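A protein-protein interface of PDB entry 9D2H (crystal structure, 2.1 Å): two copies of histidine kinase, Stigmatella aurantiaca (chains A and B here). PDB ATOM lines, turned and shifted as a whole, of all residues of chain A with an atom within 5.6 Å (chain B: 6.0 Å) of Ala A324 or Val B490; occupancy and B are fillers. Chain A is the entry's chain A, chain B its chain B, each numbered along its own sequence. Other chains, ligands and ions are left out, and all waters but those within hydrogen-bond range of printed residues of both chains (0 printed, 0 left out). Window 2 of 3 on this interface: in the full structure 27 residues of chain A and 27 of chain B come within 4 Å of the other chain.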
ATOM      1  N   LEU A 319      32.908   8.930  18.332  1.00  0.00           N
ATOM      2  CA  LEU A 319      33.174   7.500  18.484  1.00  0.00           C
ATOM      3  C   LEU A 319      32.012   6.809  19.183  1.00  0.00           C
ATOM      4  O   LEU A 319      31.457   5.835  18.668  1.00  0.00           O
ATOM      5  CB  LEU A 319      34.464   7.281  19.271  1.00  0.00           C
ATOM      6  CG  LEU A 319      35.762   7.652  18.568  1.00  0.00           C
ATOM      7  CD1 LEU A 319      36.965   7.158  19.356  1.00  0.00           C
ATOM      8  CD2 LEU A 319      35.749   7.065  17.174  1.00  0.00           C
ATOM      9  N   LEU A 320      31.636   7.327  20.364  1.00  0.00           N
ATOM     10  CA  LEU A 320      30.466   6.860  21.114  1.00  0.00           C
ATOM     11  C   LEU A 320      29.204   6.841  20.274  1.00  0.00           C
ATOM     12  O   LEU A 320      28.403   5.902  20.367  1.00  0.00           O
ATOM     13  CB  LEU A 320      30.240   7.752  22.332  1.00  0.00           C
ATOM     14  CG  LEU A 320      31.160   7.405  23.487  1.00  0.00           C
ATOM     15  CD1 LEU A 320      31.033   8.423  24.596  1.00  0.00           C
ATOM     16  CD2 LEU A 320      30.793   6.007  23.952  1.00  0.00           C
ATOM     17  N   GLY A 321      28.985   7.890  19.479  1.00  0.00           N
ATOM     18  CA  GLY A 321      27.822   7.913  18.619  1.00  0.00           C
ATOM     19  C   GLY A 321      27.831   6.788  17.609  1.00  0.00           C
ATOM     20  O   GLY A 321      26.777   6.235  17.277  1.00  0.00           O
ATOM     21  N   GLN A 322      29.016   6.416  17.124  1.00  0.00           N
ATOM     22  CA  GLN A 322      29.102   5.317  16.166  1.00  0.00           C
ATOM     23  C   GLN A 322      29.109   3.942  16.841  1.00  0.00           C
ATOM     24  O   GLN A 322      28.714   2.952  16.215  1.00  0.00           O
ATOM     25  CB  GLN A 322      30.334   5.509  15.287  1.00  0.00           C
ATOM     26  CG  GLN A 322      30.195   6.718  14.362  1.00  0.00           C
ATOM     27  CD  GLN A 322      31.537   7.267  13.872  1.00  0.00           C
ATOM     28  OE1 GLN A 322      32.600   6.683  14.134  1.00  0.00           O
ATOM     29  NE2 GLN A 322      31.491   8.402  13.164  1.00  0.00           N
ATOM     30  N   LEU A 323      29.533   3.846  18.103  1.00  0.00           N
ATOM     31  CA  LEU A 323      29.330   2.600  18.830  1.00  0.00           C
ATOM     32  C   LEU A 323      27.846   2.312  19.017  1.00  0.00           C
ATOM     33  O   LEU A 323      27.408   1.165  18.880  1.00  0.00           O
ATOM     34  CB  LEU A 323      30.039   2.644  20.182  1.00  0.00           C
ATOM     35  CG  LEU A 323      31.550   2.402  20.105  1.00  0.00           C
ATOM     36  CD1 LEU A 323      32.166   2.408  21.470  1.00  0.00           C
ATOM     37  CD2 LEU A 323      31.839   1.087  19.438  1.00  0.00           C
ATOM     38  N   ALA A 324      27.052   3.342  19.322  1.00  0.00           N
ATOM     39  CA  ALA A 324      25.640   3.120  19.614  1.00  0.00           C
ATOM     40  C   ALA A 324      24.893   2.606  18.387  1.00  0.00           C
ATOM     41  O   ALA A 324      23.963   1.802  18.508  1.00  0.00           O
ATOM     42  CB  ALA A 324      25.002   4.407  20.140  1.00  0.00           C
ATOM     43  N   THR A 325      25.287   3.050  17.196  1.00  0.00           N
ATOM     44  CA  THR A 325      24.633   2.558  15.989  1.00  0.00           C
ATOM     45  C   THR A 325      25.013   1.112  15.701  1.00  0.00           C
ATOM     46  O   THR A 325      24.197   0.349  15.171  1.00  0.00           O
ATOM     47  CB  THR A 325      24.987   3.451  14.799  1.00  0.00           C
ATOM     48  OG1 THR A 325      24.547   4.790  15.064  1.00  0.00           O
ATOM     49  CG2 THR A 325      24.322   2.943  13.532  1.00  0.00           C
ATOM     50  N   ALA A 326      26.237   0.717  16.041  1.00  0.00           N
ATOM     51  CA  ALA A 326      26.640  -0.668  15.847  1.00  0.00           C
ATOM     52  C   ALA A 326      25.837  -1.594  16.750  1.00  0.00           C
ATOM     53  O   ALA A 326      25.391  -2.664  16.321  1.00  0.00           O
ATOM     54  CB  ALA A 326      28.138  -0.803  16.102  1.00  0.00           C
ATOM     55  N   MET A 327      25.630  -1.193  18.001  1.00  0.00           N
ATOM     56  CA  MET A 327      24.596  -1.809  18.820  1.00  0.00           C
ATOM     57  C   MET A 327      23.234  -1.421  18.261  1.00  0.00           C
ATOM     58  O   MET A 327      23.158  -0.726  17.246  1.00  0.00           O
ATOM     59  CB  MET A 327      24.725  -1.374  20.275  1.00  0.00           C
ATOM     60  CG  MET A 327      26.082  -1.625  20.848  1.00  0.00           C
ATOM     61  SD  MET A 327      26.332  -0.712  22.368  1.00  0.00           S
ATOM     62  CE  MET A 327      27.948  -0.006  22.027  1.00  0.00           C
ATOM     63  N   GLY A 328      22.150  -1.851  18.898  1.00  0.00           N
ATOM     64  CA  GLY A 328      20.835  -1.567  18.347  1.00  0.00           C
ATOM     65  C   GLY A 328      20.731  -2.024  16.904  1.00  0.00           C
ATOM     66  O   GLY A 328      19.878  -1.557  16.143  1.00  0.00           O
ATOM     67  N   ALA A 488      26.691   3.337  27.947  1.00  0.00           N
ATOM     68  CA  ALA A 488      26.141   2.492  26.890  1.00  0.00           C
ATOM     69  C   ALA A 488      25.941   1.057  27.367  1.00  0.00           C
ATOM     70  O   ALA A 488      24.868   0.472  27.179  1.00  0.00           O
ATOM     71  CB  ALA A 488      27.053   2.528  25.663  1.00  0.00           C
ATOM     72  N   LEU B 416      16.069   6.152  17.920  1.00  0.00           N
ATOM     73  CA  LEU B 416      16.688   5.118  18.747  1.00  0.00           C
ATOM     74  C   LEU B 416      17.149   3.902  17.955  1.00  0.00           C
ATOM     75  O   LEU B 416      17.938   3.109  18.481  1.00  0.00           O
ATOM     76  CB  LEU B 416      15.715   4.654  19.837  1.00  0.00           C
ATOM     77  CG  LEU B 416      15.505   5.598  21.029  1.00  0.00           C
ATOM     78  CD1 LEU B 416      14.435   5.078  21.989  1.00  0.00           C
ATOM     79  CD2 LEU B 416      16.820   5.826  21.750  1.00  0.00           C
ATOM     80  N   ALA B 417      16.668   3.729  16.725  1.00  0.00           N
ATOM     81  CA  ALA B 417      17.018   2.636  15.831  1.00  0.00           C
ATOM     82  C   ALA B 417      17.368   3.190  14.458  1.00  0.00           C
ATOM     83  O   ALA B 417      16.902   4.271  14.088  1.00  0.00           O
ATOM     84  CB  ALA B 417      15.861   1.634  15.699  1.00  0.00           C
ATOM     85  N   PHE B 485      21.911  10.075  25.738  1.00  0.00           N
ATOM     86  CA  PHE B 485      20.785   9.264  26.201  1.00  0.00           C
ATOM     87  C   PHE B 485      20.492   8.154  25.198  1.00  0.00           C
ATOM     88  O   PHE B 485      20.397   6.974  25.559  1.00  0.00           O
ATOM     89  CB  PHE B 485      19.560  10.160  26.431  1.00  0.00           C
ATOM     90  CG  PHE B 485      18.385   9.450  27.062  1.00  0.00           C
ATOM     91  CD1 PHE B 485      18.374   9.155  28.420  1.00  0.00           C
ATOM     92  CD2 PHE B 485      17.283   9.088  26.295  1.00  0.00           C
ATOM     93  CE1 PHE B 485      17.295   8.501  29.001  1.00  0.00           C
ATOM     94  CE2 PHE B 485      16.197   8.444  26.871  1.00  0.00           C
ATOM     95  CZ  PHE B 485      16.208   8.144  28.226  1.00  0.00           C
ATOM     96  N   ARG B 486      20.412   8.520  23.918  1.00  0.00           N
ATOM     97  CA  ARG B 486      20.356   7.546  22.834  1.00  0.00           C
ATOM     98  C   ARG B 486      21.486   6.522  22.928  1.00  0.00           C
ATOM     99  O   ARG B 486      21.285   5.333  22.652  1.00  0.00           O
ATOM    100  CB  ARG B 486      20.406   8.283  21.494  1.00  0.00           C
ATOM    101  CG  ARG B 486      20.731   7.401  20.321  1.00  0.00           C
ATOM    102  CD  ARG B 486      20.828   8.190  19.037  1.00  0.00           C
ATOM    103  NE  ARG B 486      21.344   7.347  17.968  1.00  0.00           N
ATOM    104  CZ  ARG B 486      22.632   7.143  17.731  1.00  0.00           C
ATOM    105  NH1 ARG B 486      23.574   7.746  18.442  1.00  0.00           N
ATOM    106  NH2 ARG B 486      22.986   6.317  16.755  1.00  0.00           N
ATOM    107  N   GLY B 487      22.685   6.959  23.318  1.00  0.00           N
ATOM    108  CA  GLY B 487      23.802   6.032  23.400  1.00  0.00           C
ATOM    109  C   GLY B 487      23.585   4.917  24.402  1.00  0.00           C
ATOM    110  O   GLY B 487      24.066   3.798  24.207  1.00  0.00           O
ATOM    111  N   ALA B 488      22.773   5.170  25.421  1.00  0.00           N
ATOM    112  CA  ALA B 488      22.599   4.175  26.499  1.00  0.00           C
ATOM    113  C   ALA B 488      21.233   3.486  26.450  1.00  0.00           C
ATOM    114  O   ALA B 488      20.970   2.663  27.330  1.00  0.00           O
ATOM    115  CB  ALA B 488      22.782   4.868  27.812  1.00  0.00           C
ATOM    116  N   LEU B 489      20.400   3.819  25.471  1.00  0.00           N
ATOM    117  CA  LEU B 489      19.045   3.215  25.364  1.00  0.00           C
ATOM    118  C   LEU B 489      18.953   2.353  24.098  1.00  0.00           C
ATOM    119  O   LEU B 489      17.847   2.213  23.575  1.00  0.00           O
ATOM    120  CB  LEU B 489      18.013   4.347  25.353  1.00  0.00           C
ATOM    121  CG  LEU B 489      16.745   4.123  26.171  1.00  0.00           C
ATOM    122  CD1 LEU B 489      17.023   4.260  27.657  1.00  0.00           C
ATOM    123  CD2 LEU B 489      15.664   5.101  25.748  1.00  0.00           C
ATOM    124  N   VAL B 490      20.077   1.796  23.634  1.00  0.00           N
ATOM    125  CA  VAL B 490      20.087   0.938  22.412  1.00  0.00           C
ATOM    126  C   VAL B 490      20.423  -0.501  22.813  1.00  0.00           C
ATOM    127  O   VAL B 490      20.827  -0.684  23.971  1.00  0.00           O
ATOM    128  CB  VAL B 490      21.069   1.460  21.350  1.00  0.00           C
ATOM    129  CG1 VAL B 490      20.531   2.689  20.638  1.00  0.00           C
ATOM    130  CG2 VAL B 490      22.448   1.726  21.929  1.00  0.00           C
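OG1 of Thr A325 is in hydrogen-bond range of O of Gly A321 (3.5 Å).
Ala A488 touches its own counterpart, Ala B488. 1 position is printed for both chains. Of the 6 pairs that touch across the chains among the printed residues, 1 has its exchanged pair printed and touching as well.
Printed residues of chain A that touch a printed residue of chain B: Gly A321, Ala A324, Thr A325 and Ala A488. Along chain A the printed residues that touch a printed residue of chain B span positions 321 to 488. Printed residues of chain B that touch a printed residue of chain A: Arg B486, Gly B487, Ala B488 and Val B490. Hydrophobic or aromatic side chains of chain B within 4 Å of the printed part of chain A: Val B490. Among the printed residues, 6 pairs touch across the chains. Among the printed residues, no Asp or Glu carboxylate lies within 4 Å of a Lys or Arg side-chain nitrogen of the other chain.
Val B490 touches just one residue of chain A: Ala A324 (3.7 Å). Printed residues of chain A within 4 Å of Ala B488: Ala A488 (3.9 Å). Printed residues of chain B within 4 Å of Thr A325: Arg B486. Gln A322 touches none of the printed residues of chain B. Leu A320 touches none of the printed residues of chain B.
Among the printed residues, merely in contact across the chains: Gly A321 with Arg B486, Ala A324 with Gly B487, Ala A324 with Val B490, Ala A488 with Gly B487 and Ala A488 with Ala B488.
NH2 of Arg B486 is in hydrogen-bond range of OG1 of Thr A325.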
